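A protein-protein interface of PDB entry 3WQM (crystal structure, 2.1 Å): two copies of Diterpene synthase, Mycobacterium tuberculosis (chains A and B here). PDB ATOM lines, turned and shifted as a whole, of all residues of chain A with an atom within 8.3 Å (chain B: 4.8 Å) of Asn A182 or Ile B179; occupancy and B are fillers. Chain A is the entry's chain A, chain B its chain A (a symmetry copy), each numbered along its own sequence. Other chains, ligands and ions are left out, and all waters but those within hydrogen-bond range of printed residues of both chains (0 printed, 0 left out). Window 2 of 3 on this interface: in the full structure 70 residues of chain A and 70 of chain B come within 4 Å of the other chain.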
ATOM      1  N   VAL A 174      15.961   6.295 -20.035  1.00  0.00           N
ATOM      2  CA  VAL A 174      14.906   5.991 -19.077  1.00  0.00           C
ATOM      3  C   VAL A 174      15.441   6.184 -17.659  1.00  0.00           C
ATOM      4  O   VAL A 174      14.752   6.706 -16.787  1.00  0.00           O
ATOM      5  CB  VAL A 174      14.404   4.528 -19.237  1.00  0.00           C
ATOM      6  CG1 VAL A 174      13.434   4.170 -18.114  1.00  0.00           C
ATOM      7  CG2 VAL A 174      13.715   4.370 -20.575  1.00  0.00           C
ATOM      8  N   ALA A 175      16.674   5.749 -17.441  1.00  0.00           N
ATOM      9  CA  ALA A 175      17.320   5.864 -16.137  1.00  0.00           C
ATOM     10  C   ALA A 175      17.394   7.320 -15.679  1.00  0.00           C
ATOM     11  O   ALA A 175      16.967   7.660 -14.574  1.00  0.00           O
ATOM     12  CB  ALA A 175      18.729   5.260 -16.200  1.00  0.00           C
ATOM     13  N   GLN A 176      17.925   8.187 -16.538  1.00  0.00           N
ATOM     14  CA  GLN A 176      18.059   9.593 -16.191  1.00  0.00           C
ATOM     15  C   GLN A 176      16.712  10.273 -16.013  1.00  0.00           C
ATOM     16  O   GLN A 176      16.538  11.086 -15.103  1.00  0.00           O
ATOM     17  CB  GLN A 176      18.905  10.311 -17.243  1.00  0.00           C
ATOM     18  CG  GLN A 176      20.283   9.672 -17.384  1.00  0.00           C
ATOM     19  CD  GLN A 176      21.263  10.518 -18.173  1.00  0.00           C
ATOM     20  OE1 GLN A 176      22.401  10.110 -18.405  1.00  0.00           O
ATOM     21  NE2 GLN A 176      20.829  11.701 -18.585  1.00  0.00           N
ATOM     22  N   PHE A 177      15.760   9.933 -16.876  1.00  0.00           N
ATOM     23  CA  PHE A 177      14.410  10.484 -16.798  1.00  0.00           C
ATOM     24  C   PHE A 177      13.747  10.089 -15.470  1.00  0.00           C
ATOM     25  O   PHE A 177      13.065  10.896 -14.833  1.00  0.00           O
ATOM     26  CB  PHE A 177      13.547   9.946 -17.949  1.00  0.00           C
ATOM     27  CG  PHE A 177      12.078  10.254 -17.796  1.00  0.00           C
ATOM     28  CD1 PHE A 177      11.565  11.493 -18.174  1.00  0.00           C
ATOM     29  CD2 PHE A 177      11.216   9.321 -17.224  1.00  0.00           C
ATOM     30  CE1 PHE A 177      10.220  11.799 -17.982  1.00  0.00           C
ATOM     31  CE2 PHE A 177       9.870   9.614 -17.025  1.00  0.00           C
ATOM     32  CZ  PHE A 177       9.368  10.858 -17.405  1.00  0.00           C
ATOM     33  N   SER A 178      13.931   8.836 -15.069  1.00  0.00           N
ATOM     34  CA  SER A 178      13.330   8.342 -13.829  1.00  0.00           C
ATOM     35  C   SER A 178      13.928   9.013 -12.592  1.00  0.00           C
ATOM     36  O   SER A 178      13.219   9.324 -11.642  1.00  0.00           O
ATOM     37  CB  SER A 178      13.503   6.820 -13.740  1.00  0.00           C
ATOM     38  OG  SER A 178      12.876   6.193 -14.851  1.00  0.00           O
ATOM     39  N   ILE A 179      15.236   9.227 -12.617  1.00  0.00           N
ATOM     40  CA  ILE A 179      15.935   9.866 -11.512  1.00  0.00           C
ATOM     41  C   ILE A 179      15.434  11.300 -11.343  1.00  0.00           C
ATOM     42  O   ILE A 179      15.133  11.735 -10.227  1.00  0.00           O
ATOM     43  CB  ILE A 179      17.463   9.856 -11.771  1.00  0.00           C
ATOM     44  CG1 ILE A 179      17.995   8.418 -11.626  1.00  0.00           C
ATOM     45  CG2 ILE A 179      18.179  10.828 -10.824  1.00  0.00           C
ATOM     46  CD1 ILE A 179      19.449   8.247 -12.074  1.00  0.00           C
ATOM     47  N   SER A 180      15.326  12.031 -12.451  1.00  0.00           N
ATOM     48  CA  SER A 180      14.857  13.416 -12.393  1.00  0.00           C
ATOM     49  C   SER A 180      13.405  13.441 -11.964  1.00  0.00           C
ATOM     50  O   SER A 180      13.011  14.268 -11.147  1.00  0.00           O
ATOM     51  CB  SER A 180      14.996  14.100 -13.760  1.00  0.00           C
ATOM     52  OG  SER A 180      16.342  14.051 -14.205  1.00  0.00           O
ATOM     53  N   TRP A 181      12.612  12.524 -12.514  1.00  0.00           N
ATOM     54  CA  TRP A 181      11.202  12.458 -12.171  1.00  0.00           C
ATOM     55  C   TRP A 181      11.001  12.178 -10.679  1.00  0.00           C
ATOM     56  O   TRP A 181      10.133  12.767 -10.045  1.00  0.00           O
ATOM     57  CB  TRP A 181      10.498  11.377 -12.996  1.00  0.00           C
ATOM     58  CG  TRP A 181       9.021  11.297 -12.727  1.00  0.00           C
ATOM     59  CD1 TRP A 181       8.409  10.716 -11.648  1.00  0.00           C
ATOM     60  CD2 TRP A 181       7.973  11.829 -13.542  1.00  0.00           C
ATOM     61  NE1 TRP A 181       7.044  10.857 -11.744  1.00  0.00           N
ATOM     62  CE2 TRP A 181       6.747  11.535 -12.897  1.00  0.00           C
ATOM     63  CE3 TRP A 181       7.949  12.526 -14.758  1.00  0.00           C
ATOM     64  CZ2 TRP A 181       5.507  11.916 -13.426  1.00  0.00           C
ATOM     65  CZ3 TRP A 181       6.705  12.906 -15.288  1.00  0.00           C
ATOM     66  CH2 TRP A 181       5.508  12.599 -14.620  1.00  0.00           C
ATOM     67  N   ASN A 182      11.795  11.272 -10.122  1.00  0.00           N
ATOM     68  CA  ASN A 182      11.663  10.962  -8.706  1.00  0.00           C
ATOM     69  C   ASN A 182      12.086  12.162  -7.857  1.00  0.00           C
ATOM     70  O   ASN A 182      11.466  12.466  -6.844  1.00  0.00           O
ATOM     71  CB  ASN A 182      12.507   9.740  -8.340  1.00  0.00           C
ATOM     72  CG  ASN A 182      12.352   9.343  -6.882  1.00  0.00           C
ATOM     73  OD1 ASN A 182      13.213   9.625  -6.058  1.00  0.00           O
ATOM     74  ND2 ASN A 182      11.242   8.705  -6.559  1.00  0.00           N
ATOM     75  N   GLU A 183      13.136  12.848  -8.291  1.00  0.00           N
ATOM     76  CA  GLU A 183      13.640  14.013  -7.575  1.00  0.00           C
ATOM     77  C   GLU A 183      12.541  15.060  -7.423  1.00  0.00           C
ATOM     78  O   GLU A 183      12.260  15.528  -6.320  1.00  0.00           O
ATOM     79  CB  GLU A 183      14.826  14.611  -8.338  1.00  0.00           C
ATOM     80  CG  GLU A 183      16.002  15.052  -7.475  1.00  0.00           C
ATOM     81  CD  GLU A 183      15.714  16.300  -6.650  1.00  0.00           C
ATOM     82  OE1 GLU A 183      15.005  16.199  -5.620  1.00  0.00           O
ATOM     83  OE2 GLU A 183      16.202  17.385  -7.039  1.00  0.00           O
ATOM     84  N   THR A 184      11.909  15.403  -8.543  1.00  0.00           N
ATOM     85  CA  THR A 184      10.859  16.408  -8.568  1.00  0.00           C
ATOM     86  C   THR A 184       9.497  15.934  -8.078  1.00  0.00           C
ATOM     87  O   THR A 184       8.753  16.707  -7.478  1.00  0.00           O
ATOM     88  CB  THR A 184      10.691  16.990  -9.996  1.00  0.00           C
ATOM     89  OG1 THR A 184      10.289  15.950 -10.900  1.00  0.00           O
ATOM     90  CG2 THR A 184      12.007  17.583 -10.486  1.00  0.00           C
ATOM     91  N   HIS A 185       9.166  14.670  -8.319  1.00  0.00           N
ATOM     92  CA  HIS A 185       7.868  14.145  -7.910  1.00  0.00           C
ATOM     93  C   HIS A 185       7.840  13.382  -6.583  1.00  0.00           C
ATOM     94  O   HIS A 185       6.779  13.227  -5.991  1.00  0.00           O
ATOM     95  CB  HIS A 185       7.298  13.251  -9.017  1.00  0.00           C
ATOM     96  CG  HIS A 185       6.968  13.987 -10.279  1.00  0.00           C
ATOM     97  ND1 HIS A 185       5.711  14.485 -10.545  1.00  0.00           N
ATOM     98  CD2 HIS A 185       7.732  14.311 -11.347  1.00  0.00           C
ATOM     99  CE1 HIS A 185       5.714  15.078 -11.725  1.00  0.00           C
ATOM    100  NE2 HIS A 185       6.928  14.986 -12.233  1.00  0.00           N
ATOM    101  N   GLY A 186       8.992  12.900  -6.124  1.00  0.00           N
ATOM    102  CA  GLY A 186       9.031  12.164  -4.870  1.00  0.00           C
ATOM    103  C   GLY A 186       8.690  10.686  -4.994  1.00  0.00           C
ATOM    104  O   GLY A 186       8.750   9.942  -4.009  1.00  0.00           O
ATOM    105  N   LYS A 187       8.328  10.261  -6.202  1.00  0.00           N
ATOM    106  CA  LYS A 187       7.995   8.866  -6.467  1.00  0.00           C
ATOM    107  C   LYS A 187       8.444   8.483  -7.880  1.00  0.00           C
ATOM    108  O   LYS A 187       8.588   9.339  -8.761  1.00  0.00           O
ATOM    109  CB  LYS A 187       6.488   8.635  -6.317  1.00  0.00           C
ATOM    110  CG  LYS A 187       5.629   9.486  -7.236  1.00  0.00           C
ATOM    111  CD  LYS A 187       4.139   9.268  -6.974  1.00  0.00           C
ATOM    112  CE  LYS A 187       3.287  10.254  -7.777  1.00  0.00           C
ATOM    113  NZ  LYS A 187       1.825  10.125  -7.496  1.00  0.00           N
ATOM    114  N   PRO A 188       8.675   7.186  -8.116  1.00  0.00           N
ATOM    115  CA  PRO A 188       9.109   6.765  -9.449  1.00  0.00           C
ATOM    116  C   PRO A 188       8.010   6.999 -10.468  1.00  0.00           C
ATOM    117  O   PRO A 188       6.827   6.995 -10.126  1.00  0.00           O
ATOM    118  CB  PRO A 188       9.409   5.282  -9.255  1.00  0.00           C
ATOM    119  CG  PRO A 188       8.378   4.876  -8.259  1.00  0.00           C
ATOM    120  CD  PRO A 188       8.423   6.019  -7.251  1.00  0.00           C
ATOM    121  N   PRO A 189       8.380   7.243 -11.735  1.00  0.00           N
ATOM    122  CA  PRO A 189       7.329   7.458 -12.730  1.00  0.00           C
ATOM    123  C   PRO A 189       6.696   6.110 -13.048  1.00  0.00           C
ATOM    124  O   PRO A 189       7.321   5.064 -12.860  1.00  0.00           O
ATOM    125  CB  PRO A 189       8.098   8.005 -13.930  1.00  0.00           C
ATOM    126  CG  PRO A 189       9.414   7.262 -13.822  1.00  0.00           C
ATOM    127  CD  PRO A 189       9.717   7.392 -12.337  1.00  0.00           C
ATOM    128  N   ILE A 194       6.989   6.980 -18.203  1.00  0.00           N
ATOM    129  CA  ILE A 194       8.293   6.689 -18.785  1.00  0.00           C
ATOM    130  C   ILE A 194       8.194   6.789 -20.307  1.00  0.00           C
ATOM    131  O   ILE A 194       9.074   7.337 -20.971  1.00  0.00           O
ATOM    132  CB  ILE A 194       8.769   5.279 -18.379  1.00  0.00           C
ATOM    133  CG1 ILE A 194       9.149   5.282 -16.890  1.00  0.00           C
ATOM    134  CG2 ILE A 194       9.943   4.844 -19.265  1.00  0.00           C
ATOM    135  CD1 ILE A 194       9.354   3.893 -16.283  1.00  0.00           C
ATOM    136  N   ALA B 175      13.421   1.871 -13.965  1.00  0.00           N
ATOM    137  CA  ALA B 175      13.181   3.160 -13.323  1.00  0.00           C
ATOM    138  C   ALA B 175      13.514   3.111 -11.832  1.00  0.00           C
ATOM    139  O   ALA B 175      14.277   3.934 -11.324  1.00  0.00           O
ATOM    140  CB  ALA B 175      11.717   3.576 -13.521  1.00  0.00           C
ATOM    141  N   GLN B 176      12.950   2.131 -11.130  1.00  0.00           N
ATOM    142  CA  GLN B 176      13.187   2.006  -9.700  1.00  0.00           C
ATOM    143  C   GLN B 176      14.637   1.684  -9.383  1.00  0.00           C
ATOM    144  O   GLN B 176      15.201   2.218  -8.426  1.00  0.00           O
ATOM    145  CB  GLN B 176      12.245   0.958  -9.106  1.00  0.00           C
ATOM    146  CG  GLN B 176      10.784   1.307  -9.367  1.00  0.00           C
ATOM    147  CD  GLN B 176       9.811   0.485  -8.544  1.00  0.00           C
ATOM    148  OE1 GLN B 176       8.596   0.627  -8.682  1.00  0.00           O
ATOM    149  NE2 GLN B 176      10.338  -0.374  -7.684  1.00  0.00           N
ATOM    150  N   PHE B 177      15.240   0.818 -10.191  1.00  0.00           N
ATOM    151  CA  PHE B 177      16.642   0.446 -10.022  1.00  0.00           C
ATOM    152  C   PHE B 177      17.546   1.675 -10.192  1.00  0.00           C
ATOM    153  O   PHE B 177      18.516   1.862  -9.453  1.00  0.00           O
ATOM    154  CB  PHE B 177      17.046  -0.603 -11.070  1.00  0.00           C
ATOM    155  CG  PHE B 177      18.534  -0.847 -11.134  1.00  0.00           C
ATOM    156  CD1 PHE B 177      19.155  -1.709 -10.233  1.00  0.00           C
ATOM    157  CD2 PHE B 177      19.320  -0.173 -12.066  1.00  0.00           C
ATOM    158  CE1 PHE B 177      20.535  -1.893 -10.256  1.00  0.00           C
ATOM    159  CE2 PHE B 177      20.701  -0.347 -12.099  1.00  0.00           C
ATOM    160  CZ  PHE B 177      21.314  -1.211 -11.191  1.00  0.00           C
ATOM    161  N   SER B 178      17.238   2.500 -11.187  1.00  0.00           N
ATOM    162  CA  SER B 178      18.042   3.693 -11.458  1.00  0.00           C
ATOM    163  C   SER B 178      17.936   4.724 -10.335  1.00  0.00           C
ATOM    164  O   SER B 178      18.920   5.361  -9.972  1.00  0.00           O
ATOM    165  CB  SER B 178      17.609   4.318 -12.791  1.00  0.00           C
ATOM    166  OG  SER B 178      17.784   3.382 -13.847  1.00  0.00           O
ATOM    167  N   ILE B 179      16.735   4.882  -9.795  1.00  0.00           N
ATOM    168  CA  ILE B 179      16.494   5.822  -8.712  1.00  0.00           C
ATOM    169  C   ILE B 179      17.288   5.402  -7.475  1.00  0.00           C
ATOM    170  O   ILE B 179      17.953   6.229  -6.843  1.00  0.00           O
ATOM    171  CB  ILE B 179      14.979   5.881  -8.385  1.00  0.00           C
ATOM    172  CG1 ILE B 179      14.239   6.598  -9.529  1.00  0.00           C
ATOM    173  CG2 ILE B 179      14.743   6.568  -7.033  1.00  0.00           C
ATOM    174  CD1 ILE B 179      12.714   6.521  -9.424  1.00  0.00           C
ATOM    175  N   SER B 180      17.235   4.115  -7.138  1.00  0.00           N
ATOM    176  CA  SER B 180      17.960   3.615  -5.970  1.00  0.00           C
ATOM    177  C   SER B 180      19.450   3.722  -6.215  1.00  0.00           C
ATOM    178  O   SER B 180      20.200   4.124  -5.329  1.00  0.00           O
ATOM    179  CB  SER B 180      17.595   2.151  -5.683  1.00  0.00           C
ATOM    180  OG  SER B 180      16.196   2.017  -5.492  1.00  0.00           O
ATOM    181  N   TRP B 181      19.876   3.369  -7.425  1.00  0.00           N
ATOM    182  CA  TRP B 181      21.286   3.437  -7.767  1.00  0.00           C
ATOM    183  C   TRP B 181      21.821   4.867  -7.663  1.00  0.00           C
ATOM    184  O   TRP B 181      22.922   5.088  -7.175  1.00  0.00           O
ATOM    185  CB  TRP B 181      21.522   2.902  -9.182  1.00  0.00           C
ATOM    186  CG  TRP B 181      22.974   2.892  -9.575  1.00  0.00           C
ATOM    187  CD1 TRP B 181      23.728   3.963  -9.973  1.00  0.00           C
ATOM    188  CD2 TRP B 181      23.848   1.760  -9.591  1.00  0.00           C
ATOM    189  NE1 TRP B 181      25.018   3.565 -10.235  1.00  0.00           N
ATOM    190  CE2 TRP B 181      25.121   2.218 -10.009  1.00  0.00           C
ATOM    191  CE3 TRP B 181      23.681   0.400  -9.293  1.00  0.00           C
ATOM    192  CZ2 TRP B 181      26.225   1.363 -10.136  1.00  0.00           C
ATOM    193  CZ3 TRP B 181      24.787  -0.455  -9.422  1.00  0.00           C
ATOM    194  CH2 TRP B 181      26.036   0.033  -9.839  1.00  0.00           C
ATOM    195  N   ASN B 182      21.044   5.837  -8.131  1.00  0.00           N
ATOM    196  CA  ASN B 182      21.488   7.222  -8.058  1.00  0.00           C
ATOM    197  C   ASN B 182      21.545   7.685  -6.601  1.00  0.00           C
ATOM    198  O   ASN B 182      22.461   8.399  -6.204  1.00  0.00           O
ATOM    199  CB  ASN B 182      20.553   8.131  -8.858  1.00  0.00           C
ATOM    200  CG  ASN B 182      21.012   9.579  -8.859  1.00  0.00           C
ATOM    201  OD1 ASN B 182      20.473  10.411  -8.140  1.00  0.00           O
ATOM    202  ND2 ASN B 182      22.024   9.877  -9.654  1.00  0.00           N
ATOM    203  N   GLU B 183      20.571   7.258  -5.809  1.00  0.00           N
ATOM    204  CA  GLU B 183      20.510   7.626  -4.400  1.00  0.00           C
ATOM    205  C   GLU B 183      21.790   7.204  -3.685  1.00  0.00           C
ATOM    206  O   GLU B 183      22.440   8.011  -3.022  1.00  0.00           O
ATOM    207  CB  GLU B 183      19.302   6.950  -3.745  1.00  0.00           C
ATOM    208  CG  GLU B 183      18.506   7.825  -2.784  1.00  0.00           C
ATOM    209  CD  GLU B 183      19.238   8.114  -1.480  1.00  0.00           C
ATOM    210  OE1 GLU B 183      20.163   8.961  -1.474  1.00  0.00           O
ATOM    211  OE2 GLU B 183      18.882   7.486  -0.457  1.00  0.00           O
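Ala A175 touches Ser B178, and with the chains exchanged Ser A178 touches Ala B175. Ser A178 touches Ile B179, and with the chains exchanged Ile A179 touches Ser B178. Ile A179 touches Asn B182, and with the chains exchanged Asn A182 touches Ile B179. Positions printed for both chains: 175, 176, 177, 178, 179, 180, 181, 182 and 183. Of the 8 pairs that touch across the chains among the printed residues, 6 have their exchanged pair printed and touching as well.
OG of Ser A178 sits at hydrogen-bond distance from O of Val A174 (2.7 Å). N of Lys A187 sits close to ND2 of Asn A182.
Of the 9 printed residues of chain B, 4 touch a printed residue of chain A. Hydrophobic or aromatic side chains of chain B within 4 Å of the printed part of chain A: Ala B175 and Ile B179. Of the 17 printed residues of chain A, 6 touch a printed residue of chain B. Printed residues of chain A that touch a printed residue of chain B: Ala A175, Ser A178, Ile A179, Asn A182, Pro A188 and Ile A194. Hydrophobic or aromatic side chains of chain A within 4 Å of the printed part of chain B: Ala A175, Ile A179, Pro A188 and Ile A194. Among the printed residues, 8 pairs touch across the chains.
Trp A181 touches none of the printed residues of chain B. Asn A182 touches just one residue of chain B: Ile B179. Thr A184 touches none of the printed residues of chain B. Of the printed residues of chain A, Ala B175 touches Ser A178 (3.2 Å) and Ile A194 (3.6 Å). Ile B179 touches just these residues of chain A: Ser A178, Asn A182 and Pro A188. No residue of chain A comes within 4 Å of Ser B180. Printed residues of chain A within 4 Å of Asn B182: Ile A179 (3.4 Å). The nearest printed residue of chain B that does not touch Asn A182 is Glu B183 (6.5 Å). The nearest residue of chain A that does not touch Ile B179 is Ile A179 (4.2 Å). The nearest printed residue of chain A that does not touch Asn B182 is Glu A183 (6.5 Å).
Ala A175 touches Ser B178 (CB to OG, 3.2 Å). OG of Ser A178 touches CB of Ala B175 (3.2 Å). Ser A178 touches Ile B179. CG1 of Ile A179 touches O of Ser B178, 3.6 Å away. Ile A179 touches Asn B182 (CD1 to CB, 3.4 Å). Asn A182 touches Ile B179. Ile B179 touches Pro A188. CD1 of Ile A194 touches CB of Ala B175, at 3.6 Å.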
